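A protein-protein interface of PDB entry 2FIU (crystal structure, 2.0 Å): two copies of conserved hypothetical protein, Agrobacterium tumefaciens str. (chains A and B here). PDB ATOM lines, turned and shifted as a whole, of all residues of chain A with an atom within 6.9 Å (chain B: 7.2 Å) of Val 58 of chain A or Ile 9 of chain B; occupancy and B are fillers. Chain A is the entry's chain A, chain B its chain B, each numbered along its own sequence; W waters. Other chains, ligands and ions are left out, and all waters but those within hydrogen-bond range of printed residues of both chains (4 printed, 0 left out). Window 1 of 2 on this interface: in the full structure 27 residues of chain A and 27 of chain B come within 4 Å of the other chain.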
ATOM      1  N   TYR A   7     -29.006  27.502  26.201  1.00  0.00           N
ATOM      2  CA  TYR A   7     -27.552  27.317  26.072  1.00  0.00           C
ATOM      3  C   TYR A   7     -26.808  27.993  27.219  1.00  0.00           C
ATOM      4  O   TYR A   7     -26.664  29.224  27.262  1.00  0.00           O
ATOM      5  CB  TYR A   7     -27.055  27.754  24.700  1.00  0.00           C
ATOM      6  CG  TYR A   7     -27.680  26.911  23.611  1.00  0.00           C
ATOM      7  CD1 TYR A   7     -27.152  25.647  23.287  1.00  0.00           C
ATOM      8  CD2 TYR A   7     -28.813  27.336  22.949  1.00  0.00           C
ATOM      9  CE1 TYR A   7     -27.759  24.849  22.324  1.00  0.00           C
ATOM     10  CE2 TYR A   7     -29.425  26.545  21.974  1.00  0.00           C
ATOM     11  CZ  TYR A   7     -28.890  25.312  21.671  1.00  0.00           C
ATOM     12  OH  TYR A   7     -29.483  24.563  20.707  1.00  0.00           O
ATOM     13  N   TRP A   8     -26.366  27.150  28.145  1.00  0.00           N
ATOM     14  CA  TRP A   8     -25.460  27.507  29.225  1.00  0.00           C
ATOM     15  C   TRP A   8     -24.072  27.617  28.626  1.00  0.00           C
ATOM     16  O   TRP A   8     -23.529  26.643  28.082  1.00  0.00           O
ATOM     17  CB  TRP A   8     -25.539  26.411  30.289  1.00  0.00           C
ATOM     18  CG  TRP A   8     -24.592  26.385  31.492  1.00  0.00           C
ATOM     19  CD1 TRP A   8     -23.220  26.449  31.482  1.00  0.00           C
ATOM     20  CD2 TRP A   8     -24.967  26.152  32.871  1.00  0.00           C
ATOM     21  NE1 TRP A   8     -22.732  26.330  32.768  1.00  0.00           N
ATOM     22  CE2 TRP A   8     -23.780  26.137  33.634  1.00  0.00           C
ATOM     23  CE3 TRP A   8     -26.198  25.973  33.529  1.00  0.00           C
ATOM     24  CZ2 TRP A   8     -23.781  25.945  35.033  1.00  0.00           C
ATOM     25  CZ3 TRP A   8     -26.202  25.783  34.920  1.00  0.00           C
ATOM     26  CH2 TRP A   8     -25.004  25.779  35.652  1.00  0.00           C
ATOM     27  N   ILE A   9     -23.530  28.829  28.681  1.00  0.00           N
ATOM     28  CA  ILE A   9     -22.204  29.115  28.177  1.00  0.00           C
ATOM     29  C   ILE A   9     -21.322  29.598  29.336  1.00  0.00           C
ATOM     30  O   ILE A   9     -21.636  30.610  29.998  1.00  0.00           O
ATOM     31  CB  ILE A   9     -22.248  30.192  27.047  1.00  0.00           C
ATOM     32  CG1 ILE A   9     -23.204  29.740  25.920  1.00  0.00           C
ATOM     33  CG2 ILE A   9     -20.798  30.514  26.522  1.00  0.00           C
ATOM     34  CD1 ILE A   9     -23.422  30.789  24.812  1.00  0.00           C
ATOM     35  N   ALA A  10     -20.222  28.886  29.566  1.00  0.00           N
ATOM     36  CA  ALA A  10     -19.288  29.244  30.626  1.00  0.00           C
ATOM     37  C   ALA A  10     -17.916  29.533  30.033  1.00  0.00           C
ATOM     38  O   ALA A  10     -17.418  28.757  29.203  1.00  0.00           O
ATOM     39  CB  ALA A  10     -19.197  28.103  31.674  1.00  0.00           C
ATOM     40  N   GLN A  11     -17.295  30.632  30.459  1.00  0.00           N
ATOM     41  CA  GLN A  11     -15.989  30.988  29.949  1.00  0.00           C
ATOM     42  C   GLN A  11     -15.113  31.123  31.176  1.00  0.00           C
ATOM     43  O   GLN A  11     -15.420  31.926  32.052  1.00  0.00           O
ATOM     44  CB  GLN A  11     -16.056  32.303  29.181  1.00  0.00           C
ATOM     45  CG  GLN A  11     -17.183  32.387  28.109  1.00  0.00           C
ATOM     46  CD  GLN A  11     -17.371  33.802  27.581  1.00  0.00           C
ATOM     47  OE1 GLN A  11     -18.429  34.419  27.770  1.00  0.00           O
ATOM     48  NE2 GLN A  11     -16.340  34.335  26.947  1.00  0.00           N
ATOM     49  N   ASN A  37     -26.862  18.537  27.908  1.00  0.00           N
ATOM     50  CA  ASN A  37     -26.227  17.922  26.767  1.00  0.00           C
ATOM     51  C   ASN A  37     -24.977  18.713  26.390  1.00  0.00           C
ATOM     52  O   ASN A  37     -25.082  19.758  25.762  1.00  0.00           O
ATOM     53  CB  ASN A  37     -27.197  17.889  25.590  1.00  0.00           C
ATOM     54  CG  ASN A  37     -26.572  17.314  24.362  1.00  0.00           C
ATOM     55  OD1 ASN A  37     -25.671  16.482  24.451  1.00  0.00           O
ATOM     56  ND2 ASN A  37     -27.015  17.766  23.210  1.00  0.00           N
ATOM     57  N   PHE A  38     -23.805  18.235  26.806  1.00  0.00           N
ATOM     58  CA  PHE A  38     -22.561  18.974  26.565  1.00  0.00           C
ATOM     59  C   PHE A  38     -22.203  19.025  25.086  1.00  0.00           C
ATOM     60  O   PHE A  38     -22.048  17.979  24.457  1.00  0.00           O
ATOM     61  CB  PHE A  38     -21.394  18.401  27.372  1.00  0.00           C
ATOM     62  CG  PHE A  38     -21.373  18.850  28.807  1.00  0.00           C
ATOM     63  CD1 PHE A  38     -20.559  19.903  29.204  1.00  0.00           C
ATOM     64  CD2 PHE A  38     -22.159  18.212  29.765  1.00  0.00           C
ATOM     65  CE1 PHE A  38     -20.515  20.310  30.533  1.00  0.00           C
ATOM     66  CE2 PHE A  38     -22.145  18.631  31.092  1.00  0.00           C
ATOM     67  CZ  PHE A  38     -21.315  19.668  31.482  1.00  0.00           C
ATOM     68  N   LEU A  39     -22.101  20.238  24.538  1.00  0.00           N
ATOM     69  CA  LEU A  39     -21.717  20.442  23.137  1.00  0.00           C
ATOM     70  C   LEU A  39     -20.216  20.709  22.997  1.00  0.00           C
ATOM     71  O   LEU A  39     -19.585  20.245  22.072  1.00  0.00           O
ATOM     72  CB  LEU A  39     -22.531  21.573  22.488  1.00  0.00           C
ATOM     73  CG  LEU A  39     -24.065  21.401  22.486  1.00  0.00           C
ATOM     74  CD1 LEU A  39     -24.720  22.527  21.672  1.00  0.00           C
ATOM     75  CD2 LEU A  39     -24.469  20.006  21.939  1.00  0.00           C
ATOM     76  N   ALA A  40     -19.666  21.482  23.914  1.00  0.00           N
ATOM     77  CA  ALA A  40     -18.238  21.743  23.954  1.00  0.00           C
ATOM     78  C   ALA A  40     -17.853  21.789  25.420  1.00  0.00           C
ATOM     79  O   ALA A  40     -18.619  22.287  26.260  1.00  0.00           O
ATOM     80  CB  ALA A  40     -17.902  23.068  23.246  1.00  0.00           C
ATOM     81  N   ARG A  41     -16.668  21.278  25.737  1.00  0.00           N
ATOM     82  CA  ARG A  41     -16.219  21.263  27.116  1.00  0.00           C
ATOM     83  C   ARG A  41     -14.717  21.468  27.212  1.00  0.00           C
ATOM     84  O   ARG A  41     -13.954  20.514  27.376  1.00  0.00           O
ATOM     85  CB  ARG A  41     -16.632  19.962  27.787  1.00  0.00           C
ATOM     86  CG  ARG A  41     -16.493  19.986  29.281  1.00  0.00           C
ATOM     87  CD  ARG A  41     -16.842  18.633  29.827  1.00  0.00           C
ATOM     88  NE  ARG A  41     -17.309  18.743  31.195  1.00  0.00           N
ATOM     89  CZ  ARG A  41     -18.264  17.988  31.720  1.00  0.00           C
ATOM     90  NH1 ARG A  41     -18.619  18.180  32.982  1.00  0.00           N
ATOM     91  NH2 ARG A  41     -18.877  17.061  30.986  1.00  0.00           N
ATOM     92  N   GLY A  42     -14.311  22.723  27.087  1.00  0.00           N
ATOM     93  CA  GLY A  42     -12.892  23.115  27.181  1.00  0.00           C
ATOM     94  C   GLY A  42     -12.066  22.766  25.950  1.00  0.00           C
ATOM     95  O   GLY A  42     -10.837  22.756  26.022  1.00  0.00           O
ATOM     96  N   LEU A  48     -10.958  34.814  17.468  1.00  0.00           N
ATOM     97  CA  LEU A  48     -11.177  35.517  16.209  1.00  0.00           C
ATOM     98  C   LEU A  48     -11.038  37.005  16.464  1.00  0.00           C
ATOM     99  O   LEU A  48     -10.394  37.721  15.701  1.00  0.00           O
ATOM    100  CB  LEU A  48     -12.551  35.176  15.613  1.00  0.00           C
ATOM    101  CG  LEU A  48     -12.864  33.708  15.277  1.00  0.00           C
ATOM    102  CD1 LEU A  48     -14.304  33.569  14.811  1.00  0.00           C
ATOM    103  CD2 LEU A  48     -11.894  33.143  14.230  1.00  0.00           C
ATOM    104  N   ASN A  56     -13.800  26.928  27.719  1.00  0.00           N
ATOM    105  CA  ASN A  56     -15.126  27.377  27.274  1.00  0.00           C
ATOM    106  C   ASN A  56     -16.026  26.178  27.164  1.00  0.00           C
ATOM    107  O   ASN A  56     -15.640  25.147  26.593  1.00  0.00           O
ATOM    108  CB  ASN A  56     -15.017  28.147  25.954  1.00  0.00           C
ATOM    109  CG  ASN A  56     -14.109  29.367  26.082  1.00  0.00           C
ATOM    110  OD1 ASN A  56     -14.572  30.454  26.415  1.00  0.00           O
ATOM    111  ND2 ASN A  56     -12.803  29.180  25.860  1.00  0.00           N
ATOM    112  N   VAL A  57     -17.200  26.298  27.774  1.00  0.00           N
ATOM    113  CA  VAL A  57     -18.126  25.191  27.887  1.00  0.00           C
ATOM    114  C   VAL A  57     -19.421  25.665  27.288  1.00  0.00           C
ATOM    115  O   VAL A  57     -19.876  26.782  27.607  1.00  0.00           O
ATOM    116  CB  VAL A  57     -18.363  24.793  29.374  1.00  0.00           C
ATOM    117  CG1 VAL A  57     -19.202  23.528  29.486  1.00  0.00           C
ATOM    118  CG2 VAL A  57     -17.042  24.599  30.081  1.00  0.00           C
ATOM    119  N   VAL A  58     -20.011  24.820  26.424  1.00  0.00           N
ATOM    120  CA  VAL A  58     -21.348  25.083  25.844  1.00  0.00           C
ATOM    121  C   VAL A  58     -22.239  23.873  26.160  1.00  0.00           C
ATOM    122  O   VAL A  58     -21.983  22.768  25.688  1.00  0.00           O
ATOM    123  CB  VAL A  58     -21.284  25.315  24.309  1.00  0.00           C
ATOM    124  CG1 VAL A  58     -22.681  25.447  23.704  1.00  0.00           C
ATOM    125  CG2 VAL A  58     -20.430  26.551  23.938  1.00  0.00           C
ATOM    126  N   ILE A  59     -23.258  24.081  26.985  1.00  0.00           N
ATOM    127  CA  ILE A  59     -24.163  23.021  27.399  1.00  0.00           C
ATOM    128  C   ILE A  59     -25.538  23.331  26.831  1.00  0.00           C
ATOM    129  O   ILE A  59     -26.047  24.451  27.016  1.00  0.00           O
ATOM    130  CB  ILE A  59     -24.289  22.930  28.937  1.00  0.00           C
ATOM    131  CG1 ILE A  59     -22.923  22.959  29.581  1.00  0.00           C
ATOM    132  CG2 ILE A  59     -25.062  21.661  29.353  1.00  0.00           C
ATOM    133  CD1 ILE A  59     -22.930  22.957  31.120  1.00  0.00           C
ATOM    134  N   GLU A  60     -26.115  22.363  26.107  1.00  0.00           N
ATOM    135  CA  GLU A  60     -27.499  22.458  25.636  1.00  0.00           C
ATOM    136  C   GLU A  60     -28.435  21.801  26.666  1.00  0.00           C
ATOM    137  O   GLU A  60     -28.219  20.661  27.081  1.00  0.00           O
ATOM    138  CB  GLU A  60     -27.636  21.788  24.270  1.00  0.00           C
ATOM    139  CG  GLU A  60     -28.979  21.977  23.569  1.00  0.00           C
ATOM    140  CD  GLU A  60     -29.090  21.119  22.316  1.00  0.00           C
ATOM    141  OE1 GLU A  60     -29.435  19.930  22.487  1.00  0.00           O
ATOM    142  OE2 GLU A  60     -28.810  21.635  21.180  1.00  0.00           O
ATOM    143  N   MET A  92     -23.527  32.410  31.572  1.00  0.00           N
ATOM    144  CA  MET A  92     -24.810  32.915  31.151  1.00  0.00           C
ATOM    145  C   MET A  92     -25.617  31.802  30.479  1.00  0.00           C
ATOM    146  O   MET A  92     -25.061  30.769  30.077  1.00  0.00           O
ATOM    147  CB  MET A  92     -24.608  34.086  30.186  1.00  0.00           C
ATOM    148  CG  MET A  92     -24.002  33.674  28.876  1.00  0.00           C
ATOM    149  SD  MET A  92     -23.763  35.132  27.646  1.00  0.00           S
ATOM    150  CE  MET A  92     -22.343  34.341  26.504  1.00  0.00           C
ATOM    151  N   GLY B   6     -17.551  22.663  15.013  1.00  0.00           N
ATOM    152  CA  GLY B   6     -17.011  23.944  15.471  1.00  0.00           C
ATOM    153  C   GLY B   6     -18.123  24.849  15.969  1.00  0.00           C
ATOM    154  O   GLY B   6     -19.113  25.083  15.268  1.00  0.00           O
ATOM    155  N   TYR B   7     -17.981  25.353  17.186  1.00  0.00           N
ATOM    156  CA  TYR B   7     -18.939  26.295  17.738  1.00  0.00           C
ATOM    157  C   TYR B   7     -18.414  27.729  17.668  1.00  0.00           C
ATOM    158  O   TYR B   7     -17.549  28.113  18.437  1.00  0.00           O
ATOM    159  CB  TYR B   7     -19.355  25.880  19.167  1.00  0.00           C
ATOM    160  CG  TYR B   7     -20.109  24.550  19.139  1.00  0.00           C
ATOM    161  CD1 TYR B   7     -21.453  24.504  18.775  1.00  0.00           C
ATOM    162  CD2 TYR B   7     -19.453  23.349  19.364  1.00  0.00           C
ATOM    163  CE1 TYR B   7     -22.148  23.281  18.706  1.00  0.00           C
ATOM    164  CE2 TYR B   7     -20.133  22.123  19.289  1.00  0.00           C
ATOM    165  CZ  TYR B   7     -21.474  22.101  18.942  1.00  0.00           C
ATOM    166  OH  TYR B   7     -22.147  20.904  18.862  1.00  0.00           O
ATOM    167  N   TRP B   8     -18.929  28.484  16.706  1.00  0.00           N
ATOM    168  CA  TRP B   8     -18.710  29.920  16.574  1.00  0.00           C
ATOM    169  C   TRP B   8     -19.597  30.612  17.614  1.00  0.00           C
ATOM    170  O   TRP B   8     -20.848  30.436  17.655  1.00  0.00           O
ATOM    171  CB  TRP B   8     -19.071  30.325  15.137  1.00  0.00           C
ATOM    172  CG  TRP B   8     -19.094  31.798  14.695  1.00  0.00           C
ATOM    173  CD1 TRP B   8     -19.758  32.839  15.301  1.00  0.00           C
ATOM    174  CD2 TRP B   8     -18.516  32.344  13.487  1.00  0.00           C
ATOM    175  NE1 TRP B   8     -19.611  33.997  14.554  1.00  0.00           N
ATOM    176  CE2 TRP B   8     -18.833  33.726  13.454  1.00  0.00           C
ATOM    177  CE3 TRP B   8     -17.725  31.810  12.460  1.00  0.00           C
ATOM    178  CZ2 TRP B   8     -18.408  34.572  12.413  1.00  0.00           C
ATOM    179  CZ3 TRP B   8     -17.302  32.643  11.431  1.00  0.00           C
ATOM    180  CH2 TRP B   8     -17.649  34.013  11.414  1.00  0.00           C
ATOM    181  N   ILE B   9     -18.937  31.367  18.483  1.00  0.00           N
ATOM    182  CA  ILE B   9     -19.620  32.079  19.545  1.00  0.00           C
ATOM    183  C   ILE B   9     -19.259  33.559  19.451  1.00  0.00           C
ATOM    184  O   ILE B   9     -18.076  33.939  19.583  1.00  0.00           O
ATOM    185  CB  ILE B   9     -19.240  31.501  20.953  1.00  0.00           C
ATOM    186  CG1 ILE B   9     -19.656  30.039  21.064  1.00  0.00           C
ATOM    187  CG2 ILE B   9     -19.904  32.325  22.092  1.00  0.00           C
ATOM    188  CD1 ILE B   9     -18.926  29.306  22.133  1.00  0.00           C
ATOM    189  N   ALA B  10     -20.275  34.394  19.247  1.00  0.00           N
ATOM    190  CA  ALA B  10     -20.106  35.835  19.195  1.00  0.00           C
ATOM    191  C   ALA B  10     -20.896  36.498  20.329  1.00  0.00           C
ATOM    192  O   ALA B  10     -22.089  36.169  20.587  1.00  0.00           O
ATOM    193  CB  ALA B  10     -20.559  36.408  17.791  1.00  0.00           C
ATOM    194  N   GLN B  11     -20.240  37.417  21.023  1.00  0.00           N
ATOM    195  CA  GLN B  11     -20.912  38.205  22.048  1.00  0.00           C
ATOM    196  C   GLN B  11     -20.776  39.643  21.579  1.00  0.00           C
ATOM    197  O   GLN B  11     -19.659  40.088  21.389  1.00  0.00           O
ATOM    198  CB  GLN B  11     -20.248  38.010  23.401  1.00  0.00           C
ATOM    199  CG  GLN B  11     -20.028  36.548  23.761  1.00  0.00           C
ATOM    200  CD  GLN B  11     -19.033  36.340  24.885  1.00  0.00           C
ATOM    201  OE1 GLN B  11     -17.925  35.831  24.664  1.00  0.00           O
ATOM    202  NE2 GLN B  11     -19.430  36.681  26.091  1.00  0.00           N
ATOM    203  N   LEU B  39     -27.761  28.066  16.402  1.00  0.00           N
ATOM    204  CA  LEU B  39     -28.398  27.532  17.615  1.00  0.00           C
ATOM    205  C   LEU B  39     -29.096  28.631  18.471  1.00  0.00           C
ATOM    206  O   LEU B  39     -30.166  28.409  19.034  1.00  0.00           O
ATOM    207  CB  LEU B  39     -27.387  26.732  18.462  1.00  0.00           C
ATOM    208  CG  LEU B  39     -26.785  25.466  17.807  1.00  0.00           C
ATOM    209  CD1 LEU B  39     -25.885  24.742  18.778  1.00  0.00           C
ATOM    210  CD2 LEU B  39     -27.884  24.548  17.348  1.00  0.00           C
ATOM    211  N   ASN B  56     -25.992  37.688  21.830  1.00  0.00           N
ATOM    212  CA  ASN B  56     -25.125  36.502  21.879  1.00  0.00           C
ATOM    213  C   ASN B  56     -25.538  35.481  20.841  1.00  0.00           C
ATOM    214  O   ASN B  56     -26.722  35.185  20.678  1.00  0.00           O
ATOM    215  CB  ASN B  56     -25.136  35.875  23.271  1.00  0.00           C
ATOM    216  CG  ASN B  56     -24.606  36.813  24.335  1.00  0.00           C
ATOM    217  OD1 ASN B  56     -23.383  36.934  24.538  1.00  0.00           O
ATOM    218  ND2 ASN B  56     -25.522  37.509  25.009  1.00  0.00           N
ATOM    219  N   VAL B  57     -24.551  34.957  20.132  1.00  0.00           N
ATOM    220  CA  VAL B  57     -24.793  34.117  18.974  1.00  0.00           C
ATOM    221  C   VAL B  57     -23.971  32.849  19.114  1.00  0.00           C
ATOM    222  O   VAL B  57     -22.766  32.897  19.418  1.00  0.00           O
ATOM    223  CB  VAL B  57     -24.470  34.839  17.627  1.00  0.00           C
ATOM    224  CG1 VAL B  57     -24.765  33.904  16.419  1.00  0.00           C
ATOM    225  CG2 VAL B  57     -25.266  36.135  17.471  1.00  0.00           C
ATOM    226  N   VAL B  58     -24.633  31.717  18.921  1.00  0.00           N
ATOM    227  CA  VAL B  58     -23.968  30.406  18.965  1.00  0.00           C
ATOM    228  C   VAL B  58     -24.335  29.718  17.652  1.00  0.00           C
ATOM    229  O   VAL B  58     -25.535  29.505  17.378  1.00  0.00           O
ATOM    230  CB  VAL B  58     -24.433  29.518  20.137  1.00  0.00           C
ATOM    231  CG1 VAL B  58     -23.655  28.159  20.131  1.00  0.00           C
ATOM    232  CG2 VAL B  58     -24.287  30.238  21.489  1.00  0.00           C
ATOM    233  N   ILE B  59     -23.306  29.405  16.852  1.00  0.00           N
ATOM    234  CA  ILE B  59     -23.453  28.792  15.549  1.00  0.00           C
ATOM    235  C   ILE B  59     -22.670  27.475  15.522  1.00  0.00           C
ATOM    236  O   ILE B  59     -21.478  27.434  15.878  1.00  0.00           O
ATOM    237  CB  ILE B  59     -22.889  29.688  14.408  1.00  0.00           C
ATOM    238  CG1 ILE B  59     -23.333  31.138  14.563  1.00  0.00           C
ATOM    239  CG2 ILE B  59     -23.291  29.133  13.027  1.00  0.00           C
ATOM    240  CD1 ILE B  59     -22.612  32.089  13.609  1.00  0.00           C
ATOM    241  N   PHE B  61     -20.996  24.654  13.276  1.00  0.00           N
ATOM    242  CA  PHE B  61     -20.481  24.402  11.923  1.00  0.00           C
ATOM    243  C   PHE B  61     -20.111  22.919  11.861  1.00  0.00           C
ATOM    244  O   PHE B  61     -19.873  22.299  12.904  1.00  0.00           O
ATOM    245  CB  PHE B  61     -19.237  25.247  11.615  1.00  0.00           C
ATOM    246  CG  PHE B  61     -19.526  26.711  11.308  1.00  0.00           C
ATOM    247  CD1 PHE B  61     -19.716  27.134   9.997  1.00  0.00           C
ATOM    248  CD2 PHE B  61     -19.597  27.656  12.340  1.00  0.00           C
ATOM    249  CE1 PHE B  61     -19.959  28.477   9.697  1.00  0.00           C
ATOM    250  CE2 PHE B  61     -19.842  28.987  12.065  1.00  0.00           C
ATOM    251  CZ  PHE B  61     -20.013  29.409  10.732  1.00  0.00           C
ATOM    252  N   GLU B  90     -16.689  40.137  21.121  1.00  0.00           N
ATOM    253  CA  GLU B  90     -15.688  39.083  21.227  1.00  0.00           C
ATOM    254  C   GLU B  90     -16.190  37.907  20.392  1.00  0.00           C
ATOM    255  O   GLU B  90     -17.376  37.545  20.454  1.00  0.00           O
ATOM    256  CB  GLU B  90     -15.507  38.615  22.676  1.00  0.00           C
ATOM    257  CG  GLU B  90     -14.812  39.613  23.617  1.00  0.00           C
ATOM    258  CD  GLU B  90     -15.723  40.754  24.045  1.00  0.00           C
ATOM    259  OE1 GLU B  90     -16.845  40.488  24.560  1.00  0.00           O
ATOM    260  OE2 GLU B  90     -15.314  41.931  23.853  1.00  0.00           O
ATOM    261  N   MET B  91     -15.305  37.297  19.622  1.00  0.00           N
ATOM    262  CA  MET B  91     -15.716  36.164  18.820  1.00  0.00           C
ATOM    263  C   MET B  91     -14.674  35.095  18.882  1.00  0.00           C
ATOM    264  O   MET B  91     -13.484  35.395  18.924  1.00  0.00           O
ATOM    265  CB  MET B  91     -15.942  36.597  17.387  1.00  0.00           C
ATOM    266  CG  MET B  91     -17.050  37.623  17.273  1.00  0.00           C
ATOM    267  SD  MET B  91     -17.139  38.152  15.508  1.00  0.00           S
ATOM    268  CE  MET B  91     -17.922  36.605  14.801  1.00  0.00           C
ATOM    269  N   MET B  92     -15.130  33.845  18.885  1.00  0.00           N
ATOM    270  CA  MET B  92     -14.230  32.712  18.994  1.00  0.00           C
ATOM    271  C   MET B  92     -14.864  31.454  18.404  1.00  0.00           C
ATOM    272  O   MET B  92     -16.094  31.372  18.237  1.00  0.00           O
ATOM    273  CB  MET B  92     -13.869  32.476  20.472  1.00  0.00           C
ATOM    274  CG  MET B  92     -14.963  31.818  21.275  1.00  0.00           C
ATOM    275  SD  MET B  92     -14.556  31.738  23.169  1.00  0.00           S
ATOM    276  CE  MET B  92     -16.444  31.808  23.851  1.00  0.00           C
ATOM    277  N   ILE B  93     -14.015  30.489  18.085  1.00  0.00           N
ATOM    278  CA  ILE B  93     -14.458  29.146  17.737  1.00  0.00           C
ATOM    279  C   ILE B  93     -13.970  28.185  18.839  1.00  0.00           C
ATOM    280  O   ILE B  93     -12.789  28.182  19.200  1.00  0.00           O
ATOM    281  CB  ILE B  93     -13.987  28.737  16.304  1.00  0.00           C
ATOM    282  CG1 ILE B  93     -14.557  29.714  15.274  1.00  0.00           C
ATOM    283  CG2 ILE B  93     -14.428  27.311  15.955  1.00  0.00           C
ATOM    284  CD1 ILE B  93     -13.775  29.833  13.983  1.00  0.00           C
ATOM    285  N   VAL B  94     -14.891  27.393  19.383  1.00  0.00           N
ATOM    286  CA  VAL B  94     -14.550  26.335  20.333  1.00  0.00           C
ATOM    287  C   VAL B  94     -14.803  24.997  19.646  1.00  0.00           C
ATOM    288  O   VAL B  94     -15.852  24.793  19.043  1.00  0.00           O
ATOM    289  CB  VAL B  94     -15.459  26.412  21.571  1.00  0.00           C
ATOM    290  CG1 VAL B  94     -15.038  25.363  22.631  1.00  0.00           C
ATOM    291  CG2 VAL B  94     -15.432  27.820  22.140  1.00  0.00           C
ATOM    292  N   ILE B  97     -17.152  18.537  21.492  1.00  0.00           N
ATOM    293  CA  ILE B  97     -16.686  17.285  22.101  1.00  0.00           C
ATOM    294  C   ILE B  97     -16.418  16.208  21.044  1.00  0.00           C
ATOM    295  O   ILE B  97     -17.077  16.175  20.009  1.00  0.00           O
ATOM    296  CB  ILE B  97     -17.643  16.761  23.189  1.00  0.00           C
ATOM    297  CG1 ILE B  97     -19.015  16.433  22.582  1.00  0.00           C
ATOM    298  CG2 ILE B  97     -17.718  17.768  24.346  1.00  0.00           C
ATOM    299  CD1 ILE B  97     -19.848  15.467  23.419  1.00  0.00           C
HETATM  300  O   HOH W   1     -20.844  18.903  19.543  1.00  0.00           O
HETATM  301  O   HOH W   2     -31.475  25.687  19.349  1.00  0.00           O
HETATM  302  O   HOH W   3     -14.132  33.149  26.462  1.00  0.00           O
HETATM  303  O   HOH W   4     -21.855  37.893  26.548  1.00  0.00           O
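Phe 38 of chain A touches Ile 97 of chain B.
Leu 39 of chain A touches Tyr 7 of chain B.
Leu 39 of chain A touches Leu 39 of chain B.
Val 94 of chain B touches Ala 40 of chain A (CG1 to CB, 3.7 Å).
N of Arg 41 of chain A touches CG2 of Ile 97 of chain B, at 3.9 Å.
Asn 56 of chain A touches Val 94 of chain B.
Val 58 of chain A touches Ile 9 of chain B.
Met 92 of chain A touches Gln 11 of chain B (CE to NE2, 3.8 Å).
Of the 18 printed residues of chain A, 11 touch a printed residue of chain B.
Printed residues of chain B that touch a printed residue of chain A: Tyr 7, Ile 9, Gln 11, Leu 39, Asn 56, Val 58, Met 91, Met 92, Ile 93, Val 94 and Ile 97.
Hydrophobic or aromatic side chains of chain B that line the printed part of chain A: Tyr 7, Ile 9, Leu 39, Val 58, Met 92, Ile 93, Val 94 and Ile 97.
Among the printed residues, 17 pairs touch across the chains.
Among the printed residues, no Asp or Glu carboxylate lies within 4 Å of a Lys or Arg side-chain nitrogen of the other chain.
Of the printed residues of chain B, Ala 40 of chain A touches Val 94 (3.7 Å).
Val 58 of chain A touches one residue of chain B.
Printed residues of chain B within 4 Å of Met 92 of chain A: Gln 11 (3.8 Å) and Asn 56 (3.4 Å).
Ile 9 of chain B touches just one residue of chain A: Val 58 (3.6 Å).
Of the printed residues of chain A, Met 91 of chain B touches Leu 48.
Printed residues of chain A within 4 Å of Met 92 of chain B: Gln 11 and Asn 56.
The nearest residue of chain A that does not touch Ile 9 of chain B is Ile 9 of chain A (4.7 Å).
The nearest printed residue of chain B that does not touch Leu 48 of chain A is Met 92 of chain B (4.1 Å).
SD of Met 92 of chain A lies close to OD1 of Asn 56 of chain B, at 3.6 Å.
The backbone carbonyl oxygen of Leu 39 of chain A lies within hydrogen-bond range of the backbone NH of Ile 97 of chain B, at 3.0 Å.
The backbone carbonyl oxygen (O) of Met 91 of chain B lies within hydrogen-bond range of the backbone NH (N) of Leu 48 of chain A, at 3.0 Å.
SD of Met 92 of chain B sits close to OD1 of Asn 56 of chain A (3.5 Å).
The side-chain amide nitrogen (NE2) of Gln 11 of chain B lies within hydrogen-bond range of the side-chain amide oxygen (OE1) of Gln 11 of chain A, at 3.0 Å.
Ile 9 of chain A touches Val 58 of chain B, and with the chains exchanged Val 58 of chain A touches Ile 9 of chain B.
Gln 11 of chain A touches its own counterpart, Gln 11 of chain B.
Leu 39 of chain A touches its own counterpart, Leu 39 of chain B.
Asn 56 of chain A touches Met 92 of chain B, and with the chains exchanged Met 92 of chain A touches Asn 56 of chain B.
OH of Tyr 7 of chain A sits at hydrogen-bond distance from OE2 of Glu 60 of chain A.
The backbone NH (N) of Ile 9 of chain A lies within hydrogen-bond range of the backbone carbonyl oxygen (O) of Met 92 of chain A, 2.8 Å away.
N of Tyr 7 of chain B sits at hydrogen-bond distance from O of Val 94 of chain B (2.9 Å).
N of Ile 9 of chain B sits at hydrogen-bond distance from O of Met 92 of chain B (2.9 Å).
Water W1 bridges OH of Tyr 7 of chain B (2.5 Å) and O of Leu 39 of chain A (3.1 Å).
Water W3 lies within hydrogen-bond range of the side-chain amide nitrogen (NE2) of Gln 11 of chain A (2.6 Å), the side-chain amide oxygen (OD1) of Asn 56 of chain A (2.7 Å) and the side-chain sulfur (SD) of Met 92 of chain B (3.6 Å).
Water W2 bridges the side-chain hydroxyl (OH) of Tyr 7 of chain A and the backbone carbonyl oxygen (O) of Leu 39 of chain B.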
